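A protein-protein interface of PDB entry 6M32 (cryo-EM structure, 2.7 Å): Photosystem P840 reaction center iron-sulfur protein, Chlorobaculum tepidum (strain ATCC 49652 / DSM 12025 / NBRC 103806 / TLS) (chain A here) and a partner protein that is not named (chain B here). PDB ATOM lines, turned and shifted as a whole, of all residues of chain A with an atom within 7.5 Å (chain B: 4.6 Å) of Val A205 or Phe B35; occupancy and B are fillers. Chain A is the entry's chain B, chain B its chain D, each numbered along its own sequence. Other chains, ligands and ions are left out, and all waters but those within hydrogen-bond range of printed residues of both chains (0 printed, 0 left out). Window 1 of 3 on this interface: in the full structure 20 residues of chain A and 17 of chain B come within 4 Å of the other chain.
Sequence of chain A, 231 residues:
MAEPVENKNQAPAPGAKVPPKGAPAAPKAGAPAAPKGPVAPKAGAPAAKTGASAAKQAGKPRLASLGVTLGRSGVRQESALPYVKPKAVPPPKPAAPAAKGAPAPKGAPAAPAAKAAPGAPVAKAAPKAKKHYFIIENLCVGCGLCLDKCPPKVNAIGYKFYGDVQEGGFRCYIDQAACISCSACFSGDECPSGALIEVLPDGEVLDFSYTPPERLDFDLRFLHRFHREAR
O of Ala B54 lies within hydrogen-bond range of N of Asp A207, 3.5 Å away. O of Gly B56 lies close to OE2 of Glu A204 (3.4 Å). The backbone carbonyl oxygen (O) of Val A205 sits close to the backbone carbonyl oxygen (O) of Ala B54 (3.4 Å).
The backbone NH (N) of Ala B54 lies within hydrogen-bond range of the backbone carbonyl oxygen (O) of Lys B33 (3.1 Å). The backbone NH of Phe B35 lies within hydrogen-bond range of the backbone carbonyl oxygen of Val B52, 2.9 Å away. The backbone carbonyl oxygen (O) of Glu B50 is in hydrogen-bond range of the backbone NH (N) of Thr B37, 3.4 Å away. N of Glu A204 lies within hydrogen-bond range of OD1 of Asp A202.
Among the printed residues, pairs that only touch across the chains: Ile A136 with Trp B112 (3.9 Å), Leu A139 with Lys B33 (3.96 Å), Leu A139 with Trp B112 (3.3 Å), Gly A203 with Thr B37 (3.2 Å), Val A205 with Phe B35 (3.7 Å), Val A205 with Pro B53 (3.6 Å) and Leu A206 with Ala B54 (3.5 Å).
Printed residues of chain B within 4 Å of Val A205: Phe B35 (3.7 Å), Pro B53 (3.6 Å) and Ala B54 (3.4 Å). Printed residues of chain B within 4 Å of Asp A207: Ala B54 (3.5 Å). Of the printed residues of chain A, Phe B35 touches Val A205. Val B52 touches none of the printed residues of chain A. Of the printed residues of chain A, Pro B53 touches Val A205. Of the printed residues of chain A, Ala B54 touches Val A205, Leu A206 and Asp A207. The nearest printed residue of chain B that does not touch Val A205 is Val B52 (4.1 Å). The nearest residue of chain A that does not touch Phe B35 is Ile A136 (4.6 Å).
Of the 15 printed residues of chain A, 7 touch a printed residue of chain B. Hydrophobic or aromatic side chains of chain A that line the printed part of chain B: Ile A136, Leu A139, Val A205 and Leu A206. Of the 14 printed residues of chain B, 7 touch a printed residue of chain A. Printed residues of chain B that touch a printed residue of chain A: Lys B33, Phe B35, Thr B37, Pro B53, Ala B54, Gly B56 and Trp B112. Hydrophobic or aromatic side chains of chain B that line the printed part of chain A: Phe B35 and Trp B112. Among the printed residues, 10 pairs touch across the chains. Among the printed residues, no Asp or Glu carboxylate lies within 4 Å of a Lys or Arg side-chain nitrogen of the other chain.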
ATOM      1  N   ILE A 136      -0.752   3.674   6.669  1.00  0.00           N
ATOM      2  CA  ILE A 136      -1.973   4.400   6.330  1.00  0.00           C
ATOM      3  C   ILE A 136      -1.663   5.889   6.332  1.00  0.00           C
ATOM      4  O   ILE A 136      -1.009   6.391   7.252  1.00  0.00           O
ATOM      5  CB  ILE A 136      -3.106   4.087   7.325  1.00  0.00           C
ATOM      6  CG1 ILE A 136      -3.578   2.646   7.190  1.00  0.00           C
ATOM      7  CG2 ILE A 136      -4.286   5.016   7.102  1.00  0.00           C
ATOM      8  CD1 ILE A 136      -4.637   2.253   8.188  1.00  0.00           C
ATOM      9  N   LEU A 139      -4.300   8.224   9.006  1.00  0.00           N
ATOM     10  CA  LEU A 139      -4.148   8.026  10.442  1.00  0.00           C
ATOM     11  C   LEU A 139      -2.785   8.417  10.982  1.00  0.00           C
ATOM     12  O   LEU A 139      -2.665   8.639  12.191  1.00  0.00           O
ATOM     13  CB  LEU A 139      -4.405   6.565  10.823  1.00  0.00           C
ATOM     14  CG  LEU A 139      -5.838   6.054  10.860  1.00  0.00           C
ATOM     15  CD1 LEU A 139      -5.852   4.601  11.276  1.00  0.00           C
ATOM     16  CD2 LEU A 139      -6.642   6.877  11.848  1.00  0.00           C
ATOM     17  N   PHE A 186       6.381  -3.673  11.917  1.00  0.00           N
ATOM     18  CA  PHE A 186       5.111  -4.112  12.482  1.00  0.00           C
ATOM     19  C   PHE A 186       5.299  -4.846  13.803  1.00  0.00           C
ATOM     20  O   PHE A 186       4.574  -4.588  14.770  1.00  0.00           O
ATOM     21  CB  PHE A 186       4.367  -4.986  11.476  1.00  0.00           C
ATOM     22  CG  PHE A 186       2.930  -5.211  11.827  1.00  0.00           C
ATOM     23  CD1 PHE A 186       1.982  -4.250  11.547  1.00  0.00           C
ATOM     24  CD2 PHE A 186       2.525  -6.389  12.422  1.00  0.00           C
ATOM     25  CE1 PHE A 186       0.658  -4.453  11.866  1.00  0.00           C
ATOM     26  CE2 PHE A 186       1.201  -6.597  12.739  1.00  0.00           C
ATOM     27  CZ  PHE A 186       0.268  -5.628  12.461  1.00  0.00           C
ATOM     28  N   GLY A 194      -2.403   3.166  14.832  1.00  0.00           N
ATOM     29  CA  GLY A 194      -2.823   2.080  13.972  1.00  0.00           C
ATOM     30  C   GLY A 194      -2.659   2.379  12.501  1.00  0.00           C
ATOM     31  O   GLY A 194      -3.537   2.037  11.705  1.00  0.00           O
ATOM     32  N   ILE A 197      -0.199  -1.626   9.068  1.00  0.00           N
ATOM     33  CA  ILE A 197      -1.238  -2.640   8.942  1.00  0.00           C
ATOM     34  C   ILE A 197      -0.659  -4.036   8.734  1.00  0.00           C
ATOM     35  O   ILE A 197      -1.092  -4.996   9.377  1.00  0.00           O
ATOM     36  CB  ILE A 197      -2.234  -2.291   7.817  1.00  0.00           C
ATOM     37  CG1 ILE A 197      -1.507  -2.004   6.515  1.00  0.00           C
ATOM     38  CG2 ILE A 197      -3.054  -1.090   8.214  1.00  0.00           C
ATOM     39  CD1 ILE A 197      -2.422  -1.612   5.416  1.00  0.00           C
ATOM     40  N   GLU A 198       0.318  -4.173   7.834  1.00  0.00           N
ATOM     41  CA  GLU A 198       0.878  -5.480   7.477  1.00  0.00           C
ATOM     42  C   GLU A 198      -0.206  -6.394   6.892  1.00  0.00           C
ATOM     43  O   GLU A 198      -0.712  -7.312   7.530  1.00  0.00           O
ATOM     44  CB  GLU A 198       1.604  -6.105   8.682  1.00  0.00           C
ATOM     45  CG  GLU A 198       2.443  -7.362   8.413  1.00  0.00           C
ATOM     46  CD  GLU A 198       1.668  -8.666   8.422  1.00  0.00           C
ATOM     47  OE1 GLU A 198       0.648  -8.754   9.134  1.00  0.00           O
ATOM     48  OE2 GLU A 198       2.083  -9.608   7.716  1.00  0.00           O
ATOM     49  N   VAL A 199      -0.623  -6.042   5.674  1.00  0.00           N
ATOM     50  CA  VAL A 199      -1.534  -6.903   4.931  1.00  0.00           C
ATOM     51  C   VAL A 199      -0.904  -8.282   4.731  1.00  0.00           C
ATOM     52  O   VAL A 199       0.293  -8.413   4.451  1.00  0.00           O
ATOM     53  CB  VAL A 199      -1.910  -6.273   3.580  1.00  0.00           C
ATOM     54  CG1 VAL A 199      -2.628  -4.959   3.795  1.00  0.00           C
ATOM     55  CG2 VAL A 199      -0.679  -6.067   2.716  1.00  0.00           C
ATOM     56  N   LEU A 200      -1.720  -9.319   4.882  1.00  0.00           N
ATOM     57  CA  LEU A 200      -1.262 -10.699   4.780  1.00  0.00           C
ATOM     58  C   LEU A 200      -1.014 -11.076   3.324  1.00  0.00           C
ATOM     59  O   LEU A 200      -1.478 -10.398   2.405  1.00  0.00           O
ATOM     60  CB  LEU A 200      -2.284 -11.632   5.426  1.00  0.00           C
ATOM     61  CG  LEU A 200      -2.228 -11.820   6.946  1.00  0.00           C
ATOM     62  CD1 LEU A 200      -0.919 -12.475   7.351  1.00  0.00           C
ATOM     63  CD2 LEU A 200      -2.440 -10.519   7.706  1.00  0.00           C
ATOM     64  N   ASP A 202      -2.213 -13.254   1.282  1.00  0.00           N
ATOM     65  CA  ASP A 202      -3.316 -13.625   0.387  1.00  0.00           C
ATOM     66  C   ASP A 202      -4.322 -12.487   0.228  1.00  0.00           C
ATOM     67  O   ASP A 202      -4.455 -11.921  -0.861  1.00  0.00           O
ATOM     68  CB  ASP A 202      -3.985 -14.905   0.895  1.00  0.00           C
ATOM     69  CG  ASP A 202      -4.441 -14.798   2.338  1.00  0.00           C
ATOM     70  OD1 ASP A 202      -4.157 -13.764   2.977  1.00  0.00           O
ATOM     71  OD2 ASP A 202      -5.089 -15.743   2.830  1.00  0.00           O
ATOM     72  N   GLY A 203      -5.040 -12.144   1.296  1.00  0.00           N
ATOM     73  CA  GLY A 203      -5.883 -10.965   1.254  1.00  0.00           C
ATOM     74  C   GLY A 203      -6.105 -10.255   2.573  1.00  0.00           C
ATOM     75  O   GLY A 203      -6.753  -9.206   2.608  1.00  0.00           O
ATOM     76  N   GLU A 204      -5.562 -10.789   3.659  1.00  0.00           N
ATOM     77  CA  GLU A 204      -5.979 -10.368   4.988  1.00  0.00           C
ATOM     78  C   GLU A 204      -5.227  -9.122   5.432  1.00  0.00           C
ATOM     79  O   GLU A 204      -4.073  -8.900   5.060  1.00  0.00           O
ATOM     80  CB  GLU A 204      -5.774 -11.495   5.999  1.00  0.00           C
ATOM     81  CG  GLU A 204      -6.376 -12.816   5.558  1.00  0.00           C
ATOM     82  CD  GLU A 204      -6.334 -13.867   6.644  1.00  0.00           C
ATOM     83  OE1 GLU A 204      -5.498 -14.791   6.547  1.00  0.00           O
ATOM     84  OE2 GLU A 204      -7.136 -13.771   7.597  1.00  0.00           O
ATOM     85  N   VAL A 205      -5.902  -8.306   6.236  1.00  0.00           N
ATOM     86  CA  VAL A 205      -5.374  -7.034   6.705  1.00  0.00           C
ATOM     87  C   VAL A 205      -5.284  -7.081   8.222  1.00  0.00           C
ATOM     88  O   VAL A 205      -6.274  -7.382   8.899  1.00  0.00           O
ATOM     89  CB  VAL A 205      -6.254  -5.855   6.253  1.00  0.00           C
ATOM     90  CG1 VAL A 205      -6.000  -4.633   7.121  1.00  0.00           C
ATOM     91  CG2 VAL A 205      -6.020  -5.544   4.788  1.00  0.00           C
ATOM     92  N   LEU A 206      -4.104  -6.787   8.754  1.00  0.00           N
ATOM     93  CA  LEU A 206      -3.910  -6.642  10.186  1.00  0.00           C
ATOM     94  C   LEU A 206      -3.841  -5.164  10.550  1.00  0.00           C
ATOM     95  O   LEU A 206      -3.776  -4.289   9.688  1.00  0.00           O
ATOM     96  CB  LEU A 206      -2.640  -7.370  10.633  1.00  0.00           C
ATOM     97  CG  LEU A 206      -2.797  -8.857  10.940  1.00  0.00           C
ATOM     98  CD1 LEU A 206      -1.492  -9.446  11.433  1.00  0.00           C
ATOM     99  CD2 LEU A 206      -3.883  -9.045  11.970  1.00  0.00           C
ATOM    100  N   ASP A 207      -3.894  -4.889  11.847  1.00  0.00           N
ATOM    101  CA  ASP A 207      -3.684  -3.540  12.356  1.00  0.00           C
ATOM    102  C   ASP A 207      -2.720  -3.480  13.523  1.00  0.00           C
ATOM    103  O   ASP A 207      -2.052  -2.457  13.700  1.00  0.00           O
ATOM    104  CB  ASP A 207      -5.021  -2.914  12.783  1.00  0.00           C
ATOM    105  CG  ASP A 207      -4.871  -1.489  13.272  1.00  0.00           C
ATOM    106  OD1 ASP A 207      -4.538  -1.298  14.461  1.00  0.00           O
ATOM    107  OD2 ASP A 207      -5.088  -0.558  12.470  1.00  0.00           O
ATOM    108  N   PHE A 208      -2.616  -4.542  14.311  1.00  0.00           N
ATOM    109  CA  PHE A 208      -1.713  -4.630  15.442  1.00  0.00           C
ATOM    110  C   PHE A 208      -1.498  -6.113  15.672  1.00  0.00           C
ATOM    111  O   PHE A 208      -2.380  -6.926  15.387  1.00  0.00           O
ATOM    112  CB  PHE A 208      -2.293  -3.937  16.678  1.00  0.00           C
ATOM    113  CG  PHE A 208      -1.357  -3.874  17.844  1.00  0.00           C
ATOM    114  CD1 PHE A 208      -0.318  -2.960  17.868  1.00  0.00           C
ATOM    115  CD2 PHE A 208      -1.531  -4.706  18.929  1.00  0.00           C
ATOM    116  CE1 PHE A 208       0.536  -2.892  18.948  1.00  0.00           C
ATOM    117  CE2 PHE A 208      -0.679  -4.647  20.011  1.00  0.00           C
ATOM    118  CZ  PHE A 208       0.355  -3.737  20.020  1.00  0.00           C
ATOM    119  N   LYS B  33     -13.610  -2.349  13.654  1.00  0.00           N
ATOM    120  CA  LYS B  33     -13.286  -1.871  12.318  1.00  0.00           C
ATOM    121  C   LYS B  33     -13.200  -3.033  11.337  1.00  0.00           C
ATOM    122  O   LYS B  33     -12.748  -4.127  11.681  1.00  0.00           O
ATOM    123  CB  LYS B  33     -11.964  -1.100  12.322  1.00  0.00           C
ATOM    124  CG  LYS B  33     -11.530  -0.606  10.951  1.00  0.00           C
ATOM    125  CD  LYS B  33     -10.185   0.092  10.991  1.00  0.00           C
ATOM    126  CE  LYS B  33     -10.323   1.516  11.484  1.00  0.00           C
ATOM    127  NZ  LYS B  33      -9.053   2.269  11.323  1.00  0.00           N
ATOM    128  N   TYR B  34     -13.639  -2.784  10.104  1.00  0.00           N
ATOM    129  CA  TYR B  34     -13.567  -3.775   9.043  1.00  0.00           C
ATOM    130  C   TYR B  34     -12.944  -3.162   7.801  1.00  0.00           C
ATOM    131  O   TYR B  34     -12.960  -1.945   7.612  1.00  0.00           O
ATOM    132  CB  TYR B  34     -14.944  -4.340   8.687  1.00  0.00           C
ATOM    133  CG  TYR B  34     -15.426  -5.393   9.644  1.00  0.00           C
ATOM    134  CD1 TYR B  34     -15.845  -5.058  10.919  1.00  0.00           C
ATOM    135  CD2 TYR B  34     -15.445  -6.728   9.278  1.00  0.00           C
ATOM    136  CE1 TYR B  34     -16.282  -6.017  11.795  1.00  0.00           C
ATOM    137  CE2 TYR B  34     -15.879  -7.698  10.153  1.00  0.00           C
ATOM    138  CZ  TYR B  34     -16.298  -7.333  11.413  1.00  0.00           C
ATOM    139  OH  TYR B  34     -16.734  -8.289  12.297  1.00  0.00           O
ATOM    140  N   PHE B  35     -12.397  -4.028   6.955  1.00  0.00           N
ATOM    141  CA  PHE B  35     -11.801  -3.640   5.688  1.00  0.00           C
ATOM    142  C   PHE B  35     -12.355  -4.522   4.581  1.00  0.00           C
ATOM    143  O   PHE B  35     -12.662  -5.696   4.806  1.00  0.00           O
ATOM    144  CB  PHE B  35     -10.277  -3.768   5.728  1.00  0.00           C
ATOM    145  CG  PHE B  35      -9.588  -2.633   6.420  1.00  0.00           C
ATOM    146  CD1 PHE B  35      -9.357  -1.441   5.760  1.00  0.00           C
ATOM    147  CD2 PHE B  35      -9.162  -2.760   7.727  1.00  0.00           C
ATOM    148  CE1 PHE B  35      -8.719  -0.397   6.392  1.00  0.00           C
ATOM    149  CE2 PHE B  35      -8.525  -1.719   8.362  1.00  0.00           C
ATOM    150  CZ  PHE B  35      -8.305  -0.536   7.695  1.00  0.00           C
ATOM    151  N   ILE B  36     -12.477  -3.957   3.387  1.00  0.00           N
ATOM    152  CA  ILE B  36     -12.839  -4.725   2.203  1.00  0.00           C
ATOM    153  C   ILE B  36     -11.562  -5.172   1.510  1.00  0.00           C
ATOM    154  O   ILE B  36     -10.697  -4.350   1.191  1.00  0.00           O
ATOM    155  CB  ILE B  36     -13.725  -3.901   1.257  1.00  0.00           C
ATOM    156  CG1 ILE B  36     -15.062  -3.589   1.924  1.00  0.00           C
ATOM    157  CG2 ILE B  36     -13.948  -4.646  -0.040  1.00  0.00           C
ATOM    158  CD1 ILE B  36     -15.943  -2.670   1.119  1.00  0.00           C
ATOM    159  N   THR B  37     -11.437  -6.477   1.282  1.00  0.00           N
ATOM    160  CA  THR B  37     -10.202  -7.060   0.781  1.00  0.00           C
ATOM    161  C   THR B  37     -10.322  -7.718  -0.585  1.00  0.00           C
ATOM    162  O   THR B  37      -9.326  -7.773  -1.309  1.00  0.00           O
ATOM    163  CB  THR B  37      -9.663  -8.101   1.773  1.00  0.00           C
ATOM    164  OG1 THR B  37     -10.386  -9.327   1.619  1.00  0.00           O
ATOM    165  CG2 THR B  37      -9.816  -7.603   3.198  1.00  0.00           C
ATOM    166  N   GLU B  50     -15.451  -8.930   0.997  1.00  0.00           N
ATOM    167  CA  GLU B  50     -14.897  -9.746   2.072  1.00  0.00           C
ATOM    168  C   GLU B  50     -14.544  -8.827   3.235  1.00  0.00           C
ATOM    169  O   GLU B  50     -13.425  -8.321   3.333  1.00  0.00           O
ATOM    170  CB  GLU B  50     -13.694 -10.543   1.590  1.00  0.00           C
ATOM    171  CG  GLU B  50     -14.051 -11.589   0.553  1.00  0.00           C
ATOM    172  CD  GLU B  50     -14.923 -12.694   1.116  1.00  0.00           C
ATOM    173  OE1 GLU B  50     -14.779 -13.014   2.313  1.00  0.00           O
ATOM    174  OE2 GLU B  50     -15.755 -13.239   0.363  1.00  0.00           O
ATOM    175  N   LEU B  51     -15.515  -8.616   4.118  1.00  0.00           N
ATOM    176  CA  LEU B  51     -15.298  -7.822   5.319  1.00  0.00           C
ATOM    177  C   LEU B  51     -14.361  -8.574   6.251  1.00  0.00           C
ATOM    178  O   LEU B  51     -14.767  -9.542   6.900  1.00  0.00           O
ATOM    179  CB  LEU B  51     -16.623  -7.541   6.014  1.00  0.00           C
ATOM    180  CG  LEU B  51     -17.478  -6.448   5.393  1.00  0.00           C
ATOM    181  CD1 LEU B  51     -18.854  -6.420   6.034  1.00  0.00           C
ATOM    182  CD2 LEU B  51     -16.772  -5.136   5.545  1.00  0.00           C
ATOM    183  N   VAL B  52     -13.114  -8.137   6.325  1.00  0.00           N
ATOM    184  CA  VAL B  52     -12.129  -8.713   7.235  1.00  0.00           C
ATOM    185  C   VAL B  52     -11.981  -7.772   8.423  1.00  0.00           C
ATOM    186  O   VAL B  52     -11.776  -6.568   8.218  1.00  0.00           O
ATOM    187  CB  VAL B  52     -10.775  -8.936   6.540  1.00  0.00           C
ATOM    188  CG1 VAL B  52      -9.686  -9.165   7.570  1.00  0.00           C
ATOM    189  CG2 VAL B  52     -10.863 -10.113   5.579  1.00  0.00           C
ATOM    190  N   PRO B  53     -12.096  -8.258   9.653  1.00  0.00           N
ATOM    191  CA  PRO B  53     -11.938  -7.373  10.812  1.00  0.00           C
ATOM    192  C   PRO B  53     -10.508  -6.888  10.974  1.00  0.00           C
ATOM    193  O   PRO B  53      -9.618  -7.290  10.219  1.00  0.00           O
ATOM    194  CB  PRO B  53     -12.368  -8.258  11.987  1.00  0.00           C
ATOM    195  CG  PRO B  53     -12.128  -9.643  11.514  1.00  0.00           C
ATOM    196  CD  PRO B  53     -12.433  -9.633  10.049  1.00  0.00           C
ATOM    197  N   ALA B  54     -10.279  -6.015  11.955  1.00  0.00           N
ATOM    198  CA  ALA B  54      -8.931  -5.519  12.200  1.00  0.00           C
ATOM    199  C   ALA B  54      -7.993  -6.647  12.614  1.00  0.00           C
ATOM    200  O   ALA B  54      -6.841  -6.697  12.170  1.00  0.00           O
ATOM    201  CB  ALA B  54      -8.960  -4.426  13.266  1.00  0.00           C
ATOM    202  N   GLY B  56      -8.308  -9.760  11.787  1.00  0.00           N
ATOM    203  CA  GLY B  56      -8.105 -10.636  10.651  1.00  0.00           C
ATOM    204  C   GLY B  56      -8.142 -12.119  10.958  1.00  0.00           C
ATOM    205  O   GLY B  56      -7.132 -12.812  10.817  1.00  0.00           O
ATOM    206  N   TYR B  78     -13.868   0.267   5.452  1.00  0.00           N
ATOM    207  CA  TYR B  78     -12.940   1.099   4.702  1.00  0.00           C
ATOM    208  C   TYR B  78     -12.457   0.341   3.471  1.00  0.00           C
ATOM    209  O   TYR B  78     -12.594  -0.881   3.377  1.00  0.00           O
ATOM    210  CB  TYR B  78     -11.792   1.544   5.598  1.00  0.00           C
ATOM    211  CG  TYR B  78     -12.277   2.340   6.791  1.00  0.00           C
ATOM    212  CD1 TYR B  78     -12.481   1.727   8.017  1.00  0.00           C
ATOM    213  CD2 TYR B  78     -12.547   3.699   6.686  1.00  0.00           C
ATOM    214  CE1 TYR B  78     -12.928   2.442   9.106  1.00  0.00           C
ATOM    215  CE2 TYR B  78     -12.992   4.423   7.774  1.00  0.00           C
ATOM    216  CZ  TYR B  78     -13.181   3.788   8.981  1.00  0.00           C
ATOM    217  OH  TYR B  78     -13.626   4.495  10.072  1.00  0.00           O
ATOM    218  N   LEU B  80      -9.353   0.958   1.324  1.00  0.00           N
ATOM    219  CA  LEU B  80      -7.979   0.524   1.055  1.00  0.00           C
ATOM    220  C   LEU B  80      -7.504   0.766  -0.379  1.00  0.00           C
ATOM    221  O   LEU B  80      -7.509  -0.168  -1.180  1.00  0.00           O
ATOM    222  CB  LEU B  80      -7.842  -0.965   1.397  1.00  0.00           C
ATOM    223  CG  LEU B  80      -6.506  -1.699   1.277  1.00  0.00           C
ATOM    224  CD1 LEU B  80      -5.478  -1.130   2.209  1.00  0.00           C
ATOM    225  CD2 LEU B  80      -6.695  -3.185   1.534  1.00  0.00           C
ATOM    226  N   TRP B 112      -9.823   4.719   3.364  1.00  0.00           N
ATOM    227  CA  TRP B 112      -8.516   5.224   3.750  1.00  0.00           C
ATOM    228  C   TRP B 112      -7.653   5.344   2.501  1.00  0.00           C
ATOM    229  O   TRP B 112      -7.902   4.677   1.495  1.00  0.00           O
ATOM    230  CB  TRP B 112      -7.795   4.311   4.745  1.00  0.00           C
ATOM    231  CG  TRP B 112      -8.435   4.198   6.088  1.00  0.00           C
ATOM    232  CD1 TRP B 112      -9.236   3.190   6.501  1.00  0.00           C
ATOM    233  CD2 TRP B 112      -8.487   5.189   7.122  1.00  0.00           C
ATOM    234  NE1 TRP B 112      -9.694   3.423   7.769  1.00  0.00           N
ATOM    235  CE2 TRP B 112      -9.266   4.658   8.167  1.00  0.00           C
ATOM    236  CE3 TRP B 112      -7.919   6.450   7.284  1.00  0.00           C
ATOM    237  CZ2 TRP B 112      -9.492   5.342   9.352  1.00  0.00           C
ATOM    238  CZ3 TRP B 112      -8.144   7.128   8.464  1.00  0.00           C
ATOM    239  CH2 TRP B 112      -8.926   6.574   9.479  1.00  0.00           C
